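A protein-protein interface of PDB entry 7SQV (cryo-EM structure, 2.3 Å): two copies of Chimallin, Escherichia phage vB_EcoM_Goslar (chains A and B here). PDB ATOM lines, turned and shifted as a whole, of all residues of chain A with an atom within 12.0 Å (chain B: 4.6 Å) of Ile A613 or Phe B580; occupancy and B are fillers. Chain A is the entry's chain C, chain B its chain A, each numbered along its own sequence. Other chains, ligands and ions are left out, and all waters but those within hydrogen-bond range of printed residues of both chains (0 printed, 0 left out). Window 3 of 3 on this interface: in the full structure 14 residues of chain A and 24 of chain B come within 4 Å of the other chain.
The backbone NH (N) of Phe B580 is in hydrogen-bond range of the backbone carbonyl oxygen (O) of Ala B575 (3.5 Å).
The guanidinium group (NH2) of Arg A616 sits at hydrogen-bond distance from the backbone carbonyl oxygen (O) of Tyr A614, at 3.3 Å.
Among the printed residues, pairs that only touch across the chains: Ile A613 with Ala B576, Ile A613 with Phe B580, Ile A613 with Thr B581 and Tyr A614 with Ile B582.
The backbone carbonyl oxygen of Ile A613 lies within hydrogen-bond range of the backbone NH of Ile B582.
O of Ile B582 is in hydrogen-bond range of N of Ala A615.
No position is printed for both chains.
Of the 6 pairs that touch across the chains among the printed residues, none has its exchanged pair printed and touching as well.
Of the printed residues of chain B, Tyr A614 touches Ile B582.
Of the printed residues of chain B, Ala A615 touches Ile B582.
No residue of chain A comes within 4 Å of Leu B230.
No residue of chain A comes within 4 Å of Met B233.
No residue of chain A comes within 4 Å of Pro B238.
No residue of chain A comes within 4 Å of Ile B347.
No residue of chain A comes within 4 Å of Ile B572.
Ala B575 touches none of the printed residues of chain A.
Of chain A, only Ile A613 (3.8 Å) comes within 4 Å of Ala B576.
No residue of chain A comes within 4 Å of Ala B578.
No residue of chain A comes within 4 Å of Gly B579.
Of the printed residues of chain A, Phe B580 touches Ile A613.
Printed residues of chain A within 4 Å of Thr B581: Ile A613.
The nearest residue of chain B that does not touch Ile A613 is Ile B572 (4.1 Å).
Printed residues of chain B that touch a printed residue of chain A: Ala B576, Phe B580, Thr B581 and Ile B582.
Hydrophobic or aromatic side chains of chain B within 4 Å of the printed part of chain A: Ala B576 and Ile B582.
Hydrophobic or aromatic side chains of chain A within 4 Å of the printed part of chain B: Ile A613 and Tyr A614.
Among the printed residues, 6 pairs touch across the chains.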
ATOM      1  N   LEU A 606      24.062  17.606 -25.687  1.00  0.00           N
ATOM      2  CA  LEU A 606      23.939  16.322 -25.007  1.00  0.00           C
ATOM      3  C   LEU A 606      22.481  15.881 -25.052  1.00  0.00           C
ATOM      4  O   LEU A 606      21.610  16.543 -24.477  1.00  0.00           O
ATOM      5  CB  LEU A 606      24.431  16.421 -23.563  1.00  0.00           C
ATOM      6  CG  LEU A 606      24.217  15.193 -22.679  1.00  0.00           C
ATOM      7  CD1 LEU A 606      25.166  14.075 -23.075  1.00  0.00           C
ATOM      8  CD2 LEU A 606      24.393  15.553 -21.212  1.00  0.00           C
ATOM      9  N   GLY A 607      22.220  14.767 -25.730  1.00  0.00           N
ATOM     10  CA  GLY A 607      20.859  14.313 -25.934  1.00  0.00           C
ATOM     11  C   GLY A 607      20.288  13.462 -24.818  1.00  0.00           C
ATOM     12  O   GLY A 607      19.254  13.806 -24.238  1.00  0.00           O
ATOM     13  N   ASN A 608      20.951  12.351 -24.503  1.00  0.00           N
ATOM     14  CA  ASN A 608      20.434  11.417 -23.513  1.00  0.00           C
ATOM     15  C   ASN A 608      21.593  10.779 -22.764  1.00  0.00           C
ATOM     16  O   ASN A 608      22.734  10.768 -23.234  1.00  0.00           O
ATOM     17  CB  ASN A 608      19.557  10.339 -24.161  1.00  0.00           C
ATOM     18  CG  ASN A 608      18.096  10.473 -23.784  1.00  0.00           C
ATOM     19  OD1 ASN A 608      17.698  11.435 -23.126  1.00  0.00           O
ATOM     20  ND2 ASN A 608      17.286   9.507 -24.201  1.00  0.00           N
ATOM     21  N   ILE A 609      21.281  10.241 -21.585  1.00  0.00           N
ATOM     22  CA  ILE A 609      22.257   9.581 -20.729  1.00  0.00           C
ATOM     23  C   ILE A 609      21.734   8.195 -20.373  1.00  0.00           C
ATOM     24  O   ILE A 609      20.558   7.880 -20.560  1.00  0.00           O
ATOM     25  CB  ILE A 609      22.562  10.391 -19.451  1.00  0.00           C
ATOM     26  CG1 ILE A 609      21.299  10.549 -18.603  1.00  0.00           C
ATOM     27  CG2 ILE A 609      23.146  11.749 -19.806  1.00  0.00           C
ATOM     28  CD1 ILE A 609      21.558  11.105 -17.221  1.00  0.00           C
ATOM     29  N   SER A 610      22.636   7.363 -19.857  1.00  0.00           N
ATOM     30  CA  SER A 610      22.277   5.998 -19.495  1.00  0.00           C
ATOM     31  C   SER A 610      21.276   5.989 -18.346  1.00  0.00           C
ATOM     32  O   SER A 610      21.340   6.819 -17.435  1.00  0.00           O
ATOM     33  CB  SER A 610      23.527   5.207 -19.110  1.00  0.00           C
ATOM     34  OG  SER A 610      23.184   3.925 -18.613  1.00  0.00           O
ATOM     35  N   GLY A 611      20.347   5.038 -18.395  1.00  0.00           N
ATOM     36  CA  GLY A 611      19.319   4.902 -17.385  1.00  0.00           C
ATOM     37  C   GLY A 611      19.715   4.149 -16.138  1.00  0.00           C
ATOM     38  O   GLY A 611      18.906   4.036 -15.214  1.00  0.00           O
ATOM     39  N   ASN A 612      20.940   3.626 -16.077  1.00  0.00           N
ATOM     40  CA  ASN A 612      21.394   2.887 -14.906  1.00  0.00           C
ATOM     41  C   ASN A 612      21.801   3.792 -13.752  1.00  0.00           C
ATOM     42  O   ASN A 612      22.033   3.290 -12.646  1.00  0.00           O
ATOM     43  CB  ASN A 612      22.568   1.978 -15.280  1.00  0.00           C
ATOM     44  CG  ASN A 612      22.216   0.992 -16.374  1.00  0.00           C
ATOM     45  OD1 ASN A 612      22.902   0.905 -17.392  1.00  0.00           O
ATOM     46  ND2 ASN A 612      21.140   0.242 -16.170  1.00  0.00           N
ATOM     47  N   ILE A 613      21.895   5.106 -13.977  1.00  0.00           N
ATOM     48  CA  ILE A 613      22.271   6.033 -12.910  1.00  0.00           C
ATOM     49  C   ILE A 613      21.125   6.321 -11.955  1.00  0.00           C
ATOM     50  O   ILE A 613      21.355   6.882 -10.876  1.00  0.00           O
ATOM     51  CB  ILE A 613      22.801   7.346 -13.516  1.00  0.00           C
ATOM     52  CG1 ILE A 613      23.670   8.102 -12.507  1.00  0.00           C
ATOM     53  CG2 ILE A 613      21.650   8.219 -13.994  1.00  0.00           C
ATOM     54  CD1 ILE A 613      24.929   7.365 -12.113  1.00  0.00           C
ATOM     55  N   TYR A 614      19.901   5.942 -12.308  1.00  0.00           N
ATOM     56  CA  TYR A 614      18.728   6.219 -11.493  1.00  0.00           C
ATOM     57  C   TYR A 614      18.408   5.025 -10.604  1.00  0.00           C
ATOM     58  O   TYR A 614      18.594   3.872 -11.002  1.00  0.00           O
ATOM     59  CB  TYR A 614      17.523   6.554 -12.375  1.00  0.00           C
ATOM     60  CG  TYR A 614      17.720   7.790 -13.221  1.00  0.00           C
ATOM     61  CD1 TYR A 614      17.983   9.020 -12.634  1.00  0.00           C
ATOM     62  CD2 TYR A 614      17.652   7.726 -14.607  1.00  0.00           C
ATOM     63  CE1 TYR A 614      18.168  10.153 -13.402  1.00  0.00           C
ATOM     64  CE2 TYR A 614      17.835   8.854 -15.383  1.00  0.00           C
ATOM     65  CZ  TYR A 614      18.092  10.064 -14.776  1.00  0.00           C
ATOM     66  OH  TYR A 614      18.275  11.190 -15.544  1.00  0.00           O
ATOM     67  N   ALA A 615      17.928   5.313  -9.396  1.00  0.00           N
ATOM     68  CA  ALA A 615      17.626   4.260  -8.436  1.00  0.00           C
ATOM     69  C   ALA A 615      16.394   3.476  -8.872  1.00  0.00           C
ATOM     70  O   ALA A 615      15.364   4.059  -9.224  1.00  0.00           O
ATOM     71  CB  ALA A 615      17.410   4.858  -7.047  1.00  0.00           C
ATOM     72  N   ARG A 616      16.504   2.150  -8.845  1.00  0.00           N
ATOM     73  CA  ARG A 616      15.387   1.297  -9.222  1.00  0.00           C
ATOM     74  C   ARG A 616      14.311   1.316  -8.144  1.00  0.00           C
ATOM     75  O   ARG A 616      14.606   1.419  -6.949  1.00  0.00           O
ATOM     76  CB  ARG A 616      15.868  -0.135  -9.458  1.00  0.00           C
ATOM     77  CG  ARG A 616      16.774  -0.299 -10.667  1.00  0.00           C
ATOM     78  CD  ARG A 616      15.987  -0.238 -11.969  1.00  0.00           C
ATOM     79  NE  ARG A 616      15.916   1.112 -12.516  1.00  0.00           N
ATOM     80  CZ  ARG A 616      16.933   1.747 -13.085  1.00  0.00           C
ATOM     81  NH1 ARG A 616      18.121   1.180 -13.211  1.00  0.00           N
ATOM     82  NH2 ARG A 616      16.749   2.983 -13.542  1.00  0.00           N
ATOM     83  N   SER A 617      13.055   1.218  -8.573  1.00  0.00           N
ATOM     84  CA  SER A 617      11.941   1.191  -7.635  1.00  0.00           C
ATOM     85  C   SER A 617      11.980  -0.087  -6.806  1.00  0.00           C
ATOM     86  O   SER A 617      12.215  -1.177  -7.338  1.00  0.00           O
ATOM     87  CB  SER A 617      10.614   1.296  -8.385  1.00  0.00           C
ATOM     88  OG  SER A 617      10.566   2.473  -9.174  1.00  0.00           O
ATOM     89  N   LEU B 230      33.766   8.239  -4.726  1.00  0.00           N
ATOM     90  CA  LEU B 230      32.407   7.708  -4.700  1.00  0.00           C
ATOM     91  C   LEU B 230      32.256   6.480  -3.812  1.00  0.00           C
ATOM     92  O   LEU B 230      31.120   6.076  -3.540  1.00  0.00           O
ATOM     93  CB  LEU B 230      31.950   7.368  -6.121  1.00  0.00           C
ATOM     94  CG  LEU B 230      31.549   8.548  -7.008  1.00  0.00           C
ATOM     95  CD1 LEU B 230      31.055   8.059  -8.360  1.00  0.00           C
ATOM     96  CD2 LEU B 230      30.489   9.397  -6.323  1.00  0.00           C
ATOM     97  N   MET B 233      30.069   6.660  -0.420  1.00  0.00           N
ATOM     98  CA  MET B 233      28.616   6.757  -0.467  1.00  0.00           C
ATOM     99  C   MET B 233      27.969   5.420  -0.818  1.00  0.00           C
ATOM    100  O   MET B 233      26.853   5.381  -1.339  1.00  0.00           O
ATOM    101  CB  MET B 233      28.184   7.832  -1.463  1.00  0.00           C
ATOM    102  CG  MET B 233      29.062   9.070  -1.464  1.00  0.00           C
ATOM    103  SD  MET B 233      28.229  10.515  -2.151  1.00  0.00           S
ATOM    104  CE  MET B 233      26.735  10.544  -1.164  1.00  0.00           C
ATOM    105  N   PRO B 238      21.821   8.506  -2.089  1.00  0.00           N
ATOM    106  CA  PRO B 238      21.841   9.917  -2.487  1.00  0.00           C
ATOM    107  C   PRO B 238      20.527  10.339  -3.127  1.00  0.00           C
ATOM    108  O   PRO B 238      19.833   9.544  -3.765  1.00  0.00           O
ATOM    109  CB  PRO B 238      22.997   9.990  -3.494  1.00  0.00           C
ATOM    110  CG  PRO B 238      23.749   8.698  -3.340  1.00  0.00           C
ATOM    111  CD  PRO B 238      22.746   7.693  -2.889  1.00  0.00           C
ATOM    112  N   LEU B 344      31.620  15.599  -8.247  1.00  0.00           N
ATOM    113  CA  LEU B 344      30.380  15.025  -7.729  1.00  0.00           C
ATOM    114  C   LEU B 344      29.197  15.956  -7.972  1.00  0.00           C
ATOM    115  O   LEU B 344      28.115  15.508  -8.377  1.00  0.00           O
ATOM    116  CB  LEU B 344      30.526  14.722  -6.238  1.00  0.00           C
ATOM    117  CG  LEU B 344      29.230  14.610  -5.432  1.00  0.00           C
ATOM    118  CD1 LEU B 344      28.533  13.288  -5.716  1.00  0.00           C
ATOM    119  CD2 LEU B 344      29.502  14.769  -3.944  1.00  0.00           C
ATOM    120  N   ILE B 347      28.264  15.828 -11.648  1.00  0.00           N
ATOM    121  CA  ILE B 347      27.550  14.591 -11.956  1.00  0.00           C
ATOM    122  C   ILE B 347      26.102  14.688 -11.491  1.00  0.00           C
ATOM    123  O   ILE B 347      25.168  14.324 -12.220  1.00  0.00           O
ATOM    124  CB  ILE B 347      28.267  13.385 -11.321  1.00  0.00           C
ATOM    125  CG1 ILE B 347      29.543  13.053 -12.094  1.00  0.00           C
ATOM    126  CG2 ILE B 347      27.345  12.176 -11.268  1.00  0.00           C
ATOM    127  CD1 ILE B 347      30.387  11.979 -11.441  1.00  0.00           C
ATOM    128  N   ILE B 572      29.162   9.593 -16.899  1.00  0.00           N
ATOM    129  CA  ILE B 572      27.923   9.102 -16.301  1.00  0.00           C
ATOM    130  C   ILE B 572      27.913   7.579 -16.269  1.00  0.00           C
ATOM    131  O   ILE B 572      27.542   6.964 -15.259  1.00  0.00           O
ATOM    132  CB  ILE B 572      26.704   9.660 -17.061  1.00  0.00           C
ATOM    133  CG1 ILE B 572      26.554  11.161 -16.801  1.00  0.00           C
ATOM    134  CG2 ILE B 572      25.436   8.919 -16.663  1.00  0.00           C
ATOM    135  CD1 ILE B 572      26.165  11.498 -15.381  1.00  0.00           C
ATOM    136  N   ALA B 575      30.320   6.378 -13.573  1.00  0.00           N
ATOM    137  CA  ALA B 575      29.742   6.566 -12.247  1.00  0.00           C
ATOM    138  C   ALA B 575      28.684   5.511 -11.956  1.00  0.00           C
ATOM    139  O   ALA B 575      28.599   4.997 -10.834  1.00  0.00           O
ATOM    140  CB  ALA B 575      29.149   7.970 -12.125  1.00  0.00           C
ATOM    141  N   ALA B 576      27.862   5.179 -12.955  1.00  0.00           N
ATOM    142  CA  ALA B 576      26.874   4.120 -12.776  1.00  0.00           C
ATOM    143  C   ALA B 576      27.548   2.775 -12.528  1.00  0.00           C
ATOM    144  O   ALA B 576      27.075   1.976 -11.711  1.00  0.00           O
ATOM    145  CB  ALA B 576      25.955   4.044 -13.994  1.00  0.00           C
ATOM    146  N   ALA B 578      30.217   2.215 -10.980  1.00  0.00           N
ATOM    147  CA  ALA B 578      30.910   2.204  -9.701  1.00  0.00           C
ATOM    148  C   ALA B 578      29.975   1.979  -8.520  1.00  0.00           C
ATOM    149  O   ALA B 578      30.424   2.036  -7.371  1.00  0.00           O
ATOM    150  CB  ALA B 578      31.683   3.511  -9.509  1.00  0.00           C
ATOM    151  N   GLY B 579      28.693   1.728  -8.772  1.00  0.00           N
ATOM    152  CA  GLY B 579      27.745   1.495  -7.702  1.00  0.00           C
ATOM    153  C   GLY B 579      27.027   2.723  -7.197  1.00  0.00           C
ATOM    154  O   GLY B 579      26.433   2.672  -6.113  1.00  0.00           O
ATOM    155  N   PHE B 580      27.055   3.825  -7.941  1.00  0.00           N
ATOM    156  CA  PHE B 580      26.446   5.077  -7.518  1.00  0.00           C
ATOM    157  C   PHE B 580      25.121   5.282  -8.239  1.00  0.00           C
ATOM    158  O   PHE B 580      25.059   5.205  -9.471  1.00  0.00           O
ATOM    159  CB  PHE B 580      27.387   6.253  -7.793  1.00  0.00           C
ATOM    160  CG  PHE B 580      26.840   7.584  -7.365  1.00  0.00           C
ATOM    161  CD1 PHE B 580      26.954   8.006  -6.052  1.00  0.00           C
ATOM    162  CD2 PHE B 580      26.219   8.419  -8.281  1.00  0.00           C
ATOM    163  CE1 PHE B 580      26.454   9.232  -5.658  1.00  0.00           C
ATOM    164  CE2 PHE B 580      25.718   9.645  -7.892  1.00  0.00           C
ATOM    165  CZ  PHE B 580      25.836  10.052  -6.578  1.00  0.00           C
ATOM    166  N   THR B 581      24.066   5.539  -7.468  1.00  0.00           N
ATOM    167  CA  THR B 581      22.744   5.823  -8.004  1.00  0.00           C
ATOM    168  C   THR B 581      22.174   7.050  -7.305  1.00  0.00           C
ATOM    169  O   THR B 581      22.534   7.366  -6.169  1.00  0.00           O
ATOM    170  CB  THR B 581      21.784   4.635  -7.831  1.00  0.00           C
ATOM    171  OG1 THR B 581      21.710   4.274  -6.446  1.00  0.00           O
ATOM    172  CG2 THR B 581      22.258   3.437  -8.640  1.00  0.00           C
ATOM    173  N   ILE B 582      21.276   7.744  -8.003  1.00  0.00           N
ATOM    174  CA  ILE B 582      20.652   8.953  -7.483  1.00  0.00           C
ATOM    175  C   ILE B 582      19.158   8.903  -7.779  1.00  0.00           C
ATOM    176  O   ILE B 582      18.725   8.396  -8.818  1.00  0.00           O
ATOM    177  CB  ILE B 582      21.300  10.231  -8.067  1.00  0.00           C
ATOM    178  CG1 ILE B 582      20.821  11.475  -7.315  1.00  0.00           C
ATOM    179  CG2 ILE B 582      21.030  10.350  -9.562  1.00  0.00           C
ATOM    180  CD1 ILE B 582      21.774  12.646  -7.405  1.00  0.00           C
